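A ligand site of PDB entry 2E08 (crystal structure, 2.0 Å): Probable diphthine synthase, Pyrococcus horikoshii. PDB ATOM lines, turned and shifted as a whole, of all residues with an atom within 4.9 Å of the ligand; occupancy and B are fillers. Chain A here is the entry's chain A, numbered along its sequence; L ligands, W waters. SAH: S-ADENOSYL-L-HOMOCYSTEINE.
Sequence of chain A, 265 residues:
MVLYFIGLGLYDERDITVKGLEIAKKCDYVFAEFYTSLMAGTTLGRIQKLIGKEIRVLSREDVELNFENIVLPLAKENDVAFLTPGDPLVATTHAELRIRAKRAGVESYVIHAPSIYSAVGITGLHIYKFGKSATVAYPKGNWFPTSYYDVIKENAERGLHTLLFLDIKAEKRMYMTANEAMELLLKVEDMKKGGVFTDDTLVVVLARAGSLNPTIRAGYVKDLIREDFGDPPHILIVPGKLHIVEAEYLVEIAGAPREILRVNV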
ATOM      1  N   LEU A  10       3.425   6.674 -28.267  1.00  0.00           N
ATOM      2  CA  LEU A  10       4.420   5.834 -28.913  1.00  0.00           C
ATOM      3  C   LEU A  10       5.129   6.175 -30.224  1.00  0.00           C
ATOM      4  O   LEU A  10       6.341   6.000 -30.334  1.00  0.00           O
ATOM      5  CB  LEU A  10       3.820   4.443 -29.127  1.00  0.00           C
ATOM      6  CG  LEU A  10       3.212   3.724 -27.931  1.00  0.00           C
ATOM      7  CD1 LEU A  10       2.276   2.637 -28.431  1.00  0.00           C
ATOM      8  CD2 LEU A  10       4.297   3.146 -27.057  1.00  0.00           C
ATOM      9  N   TYR A  11       4.375   6.639 -31.211  1.00  0.00           N
ATOM     10  CA  TYR A  11       4.943   6.866 -32.534  1.00  0.00           C
ATOM     11  C   TYR A  11       4.751   8.221 -33.206  1.00  0.00           C
ATOM     12  O   TYR A  11       5.716   8.824 -33.673  1.00  0.00           O
ATOM     13  CB  TYR A  11       4.410   5.740 -33.440  1.00  0.00           C
ATOM     14  CG  TYR A  11       4.971   5.676 -34.837  1.00  0.00           C
ATOM     15  CD1 TYR A  11       6.292   5.301 -35.071  1.00  0.00           C
ATOM     16  CD2 TYR A  11       4.164   5.976 -35.937  1.00  0.00           C
ATOM     17  CE1 TYR A  11       6.806   5.218 -36.366  1.00  0.00           C
ATOM     18  CE2 TYR A  11       4.663   5.888 -37.240  1.00  0.00           C
ATOM     19  CZ  TYR A  11       5.979   5.510 -37.440  1.00  0.00           C
ATOM     20  OH  TYR A  11       6.457   5.429 -38.735  1.00  0.00           O
ATOM     21  N   THR A  36      14.181  11.197 -23.928  1.00  0.00           N
ATOM     22  CA  THR A  36      13.886   9.965 -23.209  1.00  0.00           C
ATOM     23  C   THR A  36      13.439   8.849 -24.147  1.00  0.00           C
ATOM     24  O   THR A  36      13.537   7.672 -23.806  1.00  0.00           O
ATOM     25  CB  THR A  36      12.787  10.164 -22.135  1.00  0.00           C
ATOM     26  OG1 THR A  36      11.613  10.714 -22.738  1.00  0.00           O
ATOM     27  CG2 THR A  36      13.285  11.109 -21.042  1.00  0.00           C
ATOM     28  N   SER A  37      12.942   9.209 -25.316  1.00  0.00           N
ATOM     29  CA  SER A  37      12.515   8.200 -26.273  1.00  0.00           C
ATOM     30  C   SER A  37      12.452   8.789 -27.674  1.00  0.00           C
ATOM     31  O   SER A  37      12.653   9.982 -27.860  1.00  0.00           O
ATOM     32  CB  SER A  37      11.143   7.645 -25.893  1.00  0.00           C
ATOM     33  OG  SER A  37      10.772   6.619 -26.801  1.00  0.00           O
ATOM     34  N   LEU A  38      12.161   7.931 -28.646  1.00  0.00           N
ATOM     35  CA  LEU A  38      12.084   8.363 -30.030  1.00  0.00           C
ATOM     36  C   LEU A  38      10.706   8.144 -30.641  1.00  0.00           C
ATOM     37  O   LEU A  38      10.198   7.023 -30.652  1.00  0.00           O
ATOM     38  CB  LEU A  38      13.137   7.615 -30.866  1.00  0.00           C
ATOM     39  CG  LEU A  38      13.153   7.932 -32.366  1.00  0.00           C
ATOM     40  CD1 LEU A  38      13.554   9.385 -32.590  1.00  0.00           C
ATOM     41  CD2 LEU A  38      14.139   6.991 -33.062  1.00  0.00           C
ATOM     42  N   PRO A  85       7.676  11.977 -24.863  1.00  0.00           N
ATOM     43  CA  PRO A  85       7.249  10.853 -25.699  1.00  0.00           C
ATOM     44  C   PRO A  85       6.649   9.820 -24.752  1.00  0.00           C
ATOM     45  O   PRO A  85       6.907   9.853 -23.542  1.00  0.00           O
ATOM     46  CB  PRO A  85       8.559  10.362 -26.325  1.00  0.00           C
ATOM     47  CG  PRO A  85       9.422  11.583 -26.309  1.00  0.00           C
ATOM     48  CD  PRO A  85       9.132  12.184 -24.973  1.00  0.00           C
ATOM     49  N   GLY A  86       5.855   8.894 -25.294  1.00  0.00           N
ATOM     50  CA  GLY A  86       5.242   7.850 -24.472  1.00  0.00           C
ATOM     51  C   GLY A  86       4.475   8.404 -23.293  1.00  0.00           C
ATOM     52  O   GLY A  86       3.733   9.376 -23.423  1.00  0.00           O
ATOM     53  N   ASP A  87       4.621   7.741 -22.136  1.00  0.00           N
ATOM     54  CA  ASP A  87       3.972   8.174 -20.910  1.00  0.00           C
ATOM     55  C   ASP A  87       5.067   8.950 -20.172  1.00  0.00           C
ATOM     56  O   ASP A  87       6.188   8.458 -20.024  1.00  0.00           O
ATOM     57  CB  ASP A  87       3.501   6.979 -20.088  1.00  0.00           C
ATOM     58  CG  ASP A  87       2.810   7.395 -18.793  1.00  0.00           C
ATOM     59  OD1 ASP A  87       3.491   7.949 -17.896  1.00  0.00           O
ATOM     60  OD2 ASP A  87       1.585   7.179 -18.683  1.00  0.00           O
ATOM     61  N   VAL A  90       7.046   6.918 -17.230  1.00  0.00           N
ATOM     62  CA  VAL A  90       7.506   5.535 -17.407  1.00  0.00           C
ATOM     63  C   VAL A  90       8.921   5.485 -17.957  1.00  0.00           C
ATOM     64  O   VAL A  90       9.198   6.008 -19.043  1.00  0.00           O
ATOM     65  CB  VAL A  90       6.574   4.762 -18.359  1.00  0.00           C
ATOM     66  CG1 VAL A  90       7.204   3.415 -18.712  1.00  0.00           C
ATOM     67  CG2 VAL A  90       5.218   4.553 -17.707  1.00  0.00           C
ATOM     68  N   ALA A  91       9.816   4.872 -17.203  1.00  0.00           N
ATOM     69  CA  ALA A  91      11.221   4.721 -17.614  1.00  0.00           C
ATOM     70  C   ALA A  91      11.916   6.067 -17.787  1.00  0.00           C
ATOM     71  O   ALA A  91      12.833   6.206 -18.585  1.00  0.00           O
ATOM     72  CB  ALA A  91      11.305   3.918 -18.903  1.00  0.00           C
ATOM     73  N   THR A  92      11.459   7.061 -17.037  1.00  0.00           N
ATOM     74  CA  THR A  92      12.097   8.354 -16.941  1.00  0.00           C
ATOM     75  C   THR A  92      12.268   8.708 -15.472  1.00  0.00           C
ATOM     76  O   THR A  92      11.850   7.996 -14.573  1.00  0.00           O
ATOM     77  CB  THR A  92      11.198   9.397 -17.631  1.00  0.00           C
ATOM     78  OG1 THR A  92      10.090   9.707 -16.769  1.00  0.00           O
ATOM     79  CG2 THR A  92      10.646   8.842 -18.953  1.00  0.00           C
ATOM     80  N   PRO A 114      -0.131   6.272 -24.406  1.00  0.00           N
ATOM     81  CA  PRO A 114       0.326   4.903 -24.647  1.00  0.00           C
ATOM     82  C   PRO A 114       1.825   4.784 -24.338  1.00  0.00           C
ATOM     83  O   PRO A 114       2.610   5.643 -24.728  1.00  0.00           O
ATOM     84  CB  PRO A 114       0.044   4.688 -26.137  1.00  0.00           C
ATOM     85  CG  PRO A 114      -1.128   5.578 -26.383  1.00  0.00           C
ATOM     86  CD  PRO A 114      -0.811   6.826 -25.597  1.00  0.00           C
ATOM     87  N   SER A 115       2.205   3.714 -23.640  1.00  0.00           N
ATOM     88  CA  SER A 115       3.583   3.472 -23.241  1.00  0.00           C
ATOM     89  C   SER A 115       4.088   2.146 -23.800  1.00  0.00           C
ATOM     90  O   SER A 115       3.333   1.180 -23.922  1.00  0.00           O
ATOM     91  CB  SER A 115       3.693   3.415 -21.715  1.00  0.00           C
ATOM     92  OG  SER A 115       5.005   3.049 -21.306  1.00  0.00           O
ATOM     93  N   ILE A 116       5.375   2.092 -24.136  1.00  0.00           N
ATOM     94  CA  ILE A 116       5.955   0.863 -24.659  1.00  0.00           C
ATOM     95  C   ILE A 116       5.836  -0.242 -23.616  1.00  0.00           C
ATOM     96  O   ILE A 116       5.706  -1.420 -23.933  1.00  0.00           O
ATOM     97  CB  ILE A 116       7.457   1.074 -25.024  1.00  0.00           C
ATOM     98  CG1 ILE A 116       7.986  -0.165 -25.749  1.00  0.00           C
ATOM     99  CG2 ILE A 116       8.279   1.356 -23.777  1.00  0.00           C
ATOM    100  CD1 ILE A 116       7.317  -0.432 -27.082  1.00  0.00           C
ATOM    101  N   TYR A 117       5.854   0.153 -22.343  1.00  0.00           N
ATOM    102  CA  TYR A 117       5.757  -0.800 -21.234  1.00  0.00           C
ATOM    103  C   TYR A 117       4.508  -1.677 -21.347  1.00  0.00           C
ATOM    104  O   TYR A 117       4.555  -2.866 -21.021  1.00  0.00           O
ATOM    105  CB  TYR A 117       5.786  -0.030 -19.911  1.00  0.00           C
ATOM    106  CG  TYR A 117       5.822  -0.895 -18.680  1.00  0.00           C
ATOM    107  CD1 TYR A 117       6.896  -1.754 -18.419  1.00  0.00           C
ATOM    108  CD2 TYR A 117       4.788  -0.822 -17.740  1.00  0.00           C
ATOM    109  CE1 TYR A 117       6.935  -2.526 -17.251  1.00  0.00           C
ATOM    110  CE2 TYR A 117       4.822  -1.588 -16.579  1.00  0.00           C
ATOM    111  CZ  TYR A 117       5.888  -2.428 -16.341  1.00  0.00           C
ATOM    112  OH  TYR A 117       5.881  -3.172 -15.173  1.00  0.00           O
ATOM    113  N   PHE A 165      14.523  -2.310 -22.363  1.00  0.00           N
ATOM    114  CA  PHE A 165      14.499  -1.005 -23.000  1.00  0.00           C
ATOM    115  C   PHE A 165      15.882  -0.899 -23.608  1.00  0.00           C
ATOM    116  O   PHE A 165      16.853  -1.375 -23.021  1.00  0.00           O
ATOM    117  CB  PHE A 165      14.313   0.101 -21.959  1.00  0.00           C
ATOM    118  CG  PHE A 165      12.978   0.089 -21.278  1.00  0.00           C
ATOM    119  CD1 PHE A 165      11.874   0.689 -21.866  1.00  0.00           C
ATOM    120  CD2 PHE A 165      12.820  -0.524 -20.026  1.00  0.00           C
ATOM    121  CE1 PHE A 165      10.634   0.683 -21.228  1.00  0.00           C
ATOM    122  CE2 PHE A 165      11.585  -0.528 -19.375  1.00  0.00           C
ATOM    123  CZ  PHE A 165      10.493   0.077 -19.985  1.00  0.00           C
ATOM    124  N   LEU A 166      15.984  -0.292 -24.787  1.00  0.00           N
ATOM    125  CA  LEU A 166      17.274  -0.139 -25.449  1.00  0.00           C
ATOM    126  C   LEU A 166      17.787   1.303 -25.322  1.00  0.00           C
ATOM    127  O   LEU A 166      17.012   2.261 -25.294  1.00  0.00           O
ATOM    128  CB  LEU A 166      17.165  -0.560 -26.919  1.00  0.00           C
ATOM    129  CG  LEU A 166      16.630  -1.986 -27.124  1.00  0.00           C
ATOM    130  CD1 LEU A 166      16.782  -2.382 -28.574  1.00  0.00           C
ATOM    131  CD2 LEU A 166      17.382  -2.989 -26.227  1.00  0.00           C
ATOM    132  N   ASP A 167      19.111   1.458 -25.239  1.00  0.00           N
ATOM    133  CA  ASP A 167      19.717   2.768 -25.053  1.00  0.00           C
ATOM    134  C   ASP A 167      19.455   3.772 -26.176  1.00  0.00           C
ATOM    135  O   ASP A 167      19.138   3.412 -27.306  1.00  0.00           O
ATOM    136  CB  ASP A 167      21.225   2.614 -24.844  1.00  0.00           C
ATOM    137  CG  ASP A 167      21.796   3.718 -23.975  1.00  0.00           C
ATOM    138  OD1 ASP A 167      21.035   4.627 -23.561  1.00  0.00           O
ATOM    139  OD2 ASP A 167      23.022   3.683 -23.692  1.00  0.00           O
ATOM    140  N   ILE A 168      19.580   5.046 -25.818  1.00  0.00           N
ATOM    141  CA  ILE A 168      19.378   6.133 -26.762  1.00  0.00           C
ATOM    142  C   ILE A 168      20.236   7.335 -26.396  1.00  0.00           C
ATOM    143  O   ILE A 168      20.378   7.687 -25.219  1.00  0.00           O
ATOM    144  CB  ILE A 168      17.886   6.580 -26.808  1.00  0.00           C
ATOM    145  CG1 ILE A 168      17.755   7.883 -27.608  1.00  0.00           C
ATOM    146  CG2 ILE A 168      17.348   6.751 -25.400  1.00  0.00           C
ATOM    147  CD1 ILE A 168      16.354   8.471 -27.624  1.00  0.00           C
ATOM    148  N   LEU A 206      10.222  -5.922 -31.082  1.00  0.00           N
ATOM    149  CA  LEU A 206       9.086  -5.078 -31.430  1.00  0.00           C
ATOM    150  C   LEU A 206       9.685  -3.745 -31.848  1.00  0.00           C
ATOM    151  O   LEU A 206      10.377  -3.087 -31.059  1.00  0.00           O
ATOM    152  CB  LEU A 206       8.168  -4.878 -30.210  1.00  0.00           C
ATOM    153  CG  LEU A 206       6.967  -3.947 -30.411  1.00  0.00           C
ATOM    154  CD1 LEU A 206       6.103  -4.419 -31.584  1.00  0.00           C
ATOM    155  CD2 LEU A 206       6.144  -3.908 -29.129  1.00  0.00           C
ATOM    156  N   ALA A 207       9.444  -3.346 -33.090  1.00  0.00           N
ATOM    157  CA  ALA A 207       9.998  -2.099 -33.591  1.00  0.00           C
ATOM    158  C   ALA A 207       8.905  -1.124 -33.988  1.00  0.00           C
ATOM    159  O   ALA A 207       7.974  -1.488 -34.696  1.00  0.00           O
ATOM    160  CB  ALA A 207      10.908  -2.362 -34.781  1.00  0.00           C
ATOM    161  N   ARG A 208       9.046   0.111 -33.536  1.00  0.00           N
ATOM    162  CA  ARG A 208       8.099   1.171 -33.840  1.00  0.00           C
ATOM    163  C   ARG A 208       6.672   0.852 -33.411  1.00  0.00           C
ATOM    164  O   ARG A 208       5.729   0.969 -34.194  1.00  0.00           O
ATOM    165  CB  ARG A 208       8.151   1.480 -35.347  1.00  0.00           C
ATOM    166  CG  ARG A 208       9.554   1.835 -35.865  1.00  0.00           C
ATOM    167  CD  ARG A 208       9.550   2.062 -37.380  1.00  0.00           C
ATOM    168  NE  ARG A 208       8.980   0.905 -38.077  1.00  0.00           N
ATOM    169  CZ  ARG A 208       9.564  -0.287 -38.145  1.00  0.00           C
ATOM    170  NH1 ARG A 208      10.747  -0.484 -37.558  1.00  0.00           N
ATOM    171  NH2 ARG A 208       8.953  -1.293 -38.739  1.00  0.00           N
ATOM    172  N   ALA A 209       6.510   0.434 -32.159  1.00  0.00           N
ATOM    173  CA  ALA A 209       5.190   0.149 -31.634  1.00  0.00           C
ATOM    174  C   ALA A 209       4.427   1.469 -31.774  1.00  0.00           C
ATOM    175  O   ALA A 209       5.013   2.537 -31.672  1.00  0.00           O
ATOM    176  CB  ALA A 209       5.279  -0.264 -30.165  1.00  0.00           C
ATOM    177  N   GLY A 210       3.116   1.388 -32.008  1.00  0.00           N
ATOM    178  CA  GLY A 210       2.338   2.612 -32.156  1.00  0.00           C
ATOM    179  C   GLY A 210       2.006   2.878 -33.610  1.00  0.00           C
ATOM    180  O   GLY A 210       0.946   3.417 -33.925  1.00  0.00           O
ATOM    181  N   PRO A 233      12.490   3.357 -32.969  1.00  0.00           N
ATOM    182  CA  PRO A 233      13.064   2.649 -31.822  1.00  0.00           C
ATOM    183  C   PRO A 233      12.747   1.161 -31.809  1.00  0.00           C
ATOM    184  O   PRO A 233      11.780   0.707 -32.423  1.00  0.00           O
ATOM    185  CB  PRO A 233      12.456   3.393 -30.627  1.00  0.00           C
ATOM    186  CG  PRO A 233      11.069   3.708 -31.128  1.00  0.00           C
ATOM    187  CD  PRO A 233      11.314   4.167 -32.558  1.00  0.00           C
ATOM    188  N   HIS A 234      13.573   0.408 -31.088  1.00  0.00           N
ATOM    189  CA  HIS A 234      13.408  -1.028 -30.972  1.00  0.00           C
ATOM    190  C   HIS A 234      13.357  -1.412 -29.499  1.00  0.00           C
ATOM    191  O   HIS A 234      13.914  -0.724 -28.648  1.00  0.00           O
ATOM    192  CB  HIS A 234      14.612  -1.796 -31.574  1.00  0.00           C
ATOM    193  CG  HIS A 234      14.725  -1.706 -33.056  1.00  0.00           C
ATOM    194  ND1 HIS A 234      15.716  -2.366 -33.761  1.00  0.00           N
ATOM    195  CD2 HIS A 234      13.990  -1.030 -33.984  1.00  0.00           C
ATOM    196  CE1 HIS A 234      15.581  -2.108 -35.043  1.00  0.00           C
ATOM    197  NE2 HIS A 234      14.550  -1.300 -35.213  1.00  0.00           N
ATOM    198  N   ILE A 235      12.706  -2.530 -29.228  1.00  0.00           N
ATOM    199  CA  ILE A 235      12.644  -3.046 -27.878  1.00  0.00           C
ATOM    200  C   ILE A 235      12.960  -4.523 -28.015  1.00  0.00           C
ATOM    201  O   ILE A 235      12.588  -5.147 -29.013  1.00  0.00           O
ATOM    202  CB  ILE A 235      11.236  -2.843 -27.247  1.00  0.00           C
ATOM    203  CG1 ILE A 235      11.364  -2.756 -25.738  1.00  0.00           C
ATOM    204  CG2 ILE A 235      10.323  -4.005 -27.595  1.00  0.00           C
ATOM    205  CD1 ILE A 235      12.069  -1.515 -25.271  1.00  0.00           C
HETATM  206  N   SAH L   1       8.272   6.981 -21.330  1.00  0.00           N
HETATM  207  CA  SAH L   1       8.550   6.079 -22.524  1.00  0.00           C
HETATM  208  CB  SAH L   1       9.764   5.190 -22.453  1.00  0.00           C
HETATM  209  CG  SAH L   1      11.135   5.810 -22.226  1.00  0.00           C
HETATM  210  SD  SAH L   1      12.376   4.480 -22.485  1.00  0.00           S
HETATM  211  C   SAH L   1       7.243   5.211 -22.769  1.00  0.00           C
HETATM  212  O   SAH L   1       6.275   5.363 -21.989  1.00  0.00           O
HETATM  213  OXT SAH L   1       7.272   4.385 -23.764  1.00  0.00           O
HETATM  214  C5' SAH L   1      12.709   4.693 -24.187  1.00  0.00           C
HETATM  215  C4' SAH L   1      13.086   3.296 -24.842  1.00  0.00           C
HETATM  216  O4' SAH L   1      11.882   2.481 -24.844  1.00  0.00           O
HETATM  217  C3' SAH L   1      13.555   3.363 -26.251  1.00  0.00           C
HETATM  218  O3' SAH L   1      14.966   3.568 -26.309  1.00  0.00           O
HETATM  219  C2' SAH L   1      13.051   2.011 -26.827  1.00  0.00           C
HETATM  220  O2' SAH L   1      13.965   0.938 -26.553  1.00  0.00           O
HETATM  221  C1' SAH L   1      11.671   1.831 -26.176  1.00  0.00           C
HETATM  222  N9  SAH L   1      10.650   2.410 -26.852  1.00  0.00           N
HETATM  223  C8  SAH L   1       9.922   3.575 -26.715  1.00  0.00           C
HETATM  224  N7  SAH L   1       8.992   3.766 -27.602  1.00  0.00           N
HETATM  225  C5  SAH L   1       9.078   2.621 -28.451  1.00  0.00           C
HETATM  226  C6  SAH L   1       8.327   2.231 -29.618  1.00  0.00           C
HETATM  227  N6  SAH L   1       7.328   2.947 -30.146  1.00  0.00           N
HETATM  228  N1  SAH L   1       8.714   1.026 -30.176  1.00  0.00           N
HETATM  229  C2  SAH L   1       9.716   0.251 -29.686  1.00  0.00           C
HETATM  230  N3  SAH L   1      10.454   0.599 -28.577  1.00  0.00           N
HETATM  231  C4  SAH L   1      10.086   1.788 -28.017  1.00  0.00           C
HETATM  232  O   HOH W   1      16.431   3.692 -28.702  1.00  0.00           O
HETATM  233  O   HOH W   2       9.504   9.079 -22.625  1.00  0.00           O
HETATM  234  O   HOH W   3       8.415   5.591 -32.102  1.00  0.00           O
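O of Leu 206 is in hydrogen-bond range of N of Ile 235 (3.0 Å).
OG of Ser 115 lies close to N of Tyr 117 (3.2 Å).
N of Arg 208 sits at hydrogen-bond distance from O of Pro 233 (3.0 Å).
Water W2 lies within hydrogen-bond range of the side-chain hydroxyl of Thr 36, a nitrogen (N) of the ligand and the backbone carbonyl oxygen of Pro 85.
Water W1 lies within hydrogen-bond range of O3' of the ligand (2.8 Å) and O of Asp 167 (3.1 Å).
Water W3 lies within hydrogen-bond range of O of Leu 38 (2.7 Å), O of Leu 10 (2.8 Å) and N6 of the ligand (3.5 Å).
The backbone carbonyl oxygen (O) of Asp 87 sits at hydrogen-bond distance from a nitrogen (N) of the ligand, at 2.9 Å.
OG of Ser 115 is in hydrogen-bond range of O of the ligand (2.7 Å).
An oxygen (O3') of the ligand lies within hydrogen-bond range of the backbone carbonyl oxygen (O) of Leu 166.
N of Leu 166 sits at hydrogen-bond distance from O2' of the ligand, 3.0 Å away.
O of Val 90 lies within hydrogen-bond range of N of the ligand, at 2.7 Å.
The backbone NH (N) of Ile 116 lies within hydrogen-bond range of an oxygen (OXT) of the ligand (3.0 Å).
The side-chain hydroxyl (OG) of Ser 37 lies close to a nitrogen (N7) of the ligand, at 3.5 Å.
O of Leu 10 sits at hydrogen-bond distance from N6 of the ligand, at 3.2 Å.
N of Asp 87 sits at hydrogen-bond distance from O of the ligand.
O2' of the ligand lies within hydrogen-bond range of O of His 234.
N1 of the ligand sits at hydrogen-bond distance from N of Ala 209, 3.0 Å away.
N of Arg 208 sits at hydrogen-bond distance from N1 of the ligand, at 3.5 Å.
O of Ala 209 lies within hydrogen-bond range of N6 of the ligand, 2.8 Å away.
A sulfur (SD) of the ligand lies close to the backbone carbonyl oxygen (O) of Thr 36, 3.6 Å away.
Residues that only touch the ligand: Ile 235 (3.4 Å), Pro 233 (3.5 Å), Phe 165 (3.5 Å), Gly 86 (3.7 Å), Leu 206 (3.7 Å), Ala 91 (3.8 Å), Thr 92 (3.8 Å) and Pro 85 (3.9 Å).
Hydrophobic or aromatic side chains that line the ligand: Leu 10, Val 90, Ala 91, Ile 116, Phe 165, Leu 166, Ala 209, Pro 233 and Ile 235.
Of the 27 residues printed, 19 come within 4 Å of the ligand.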
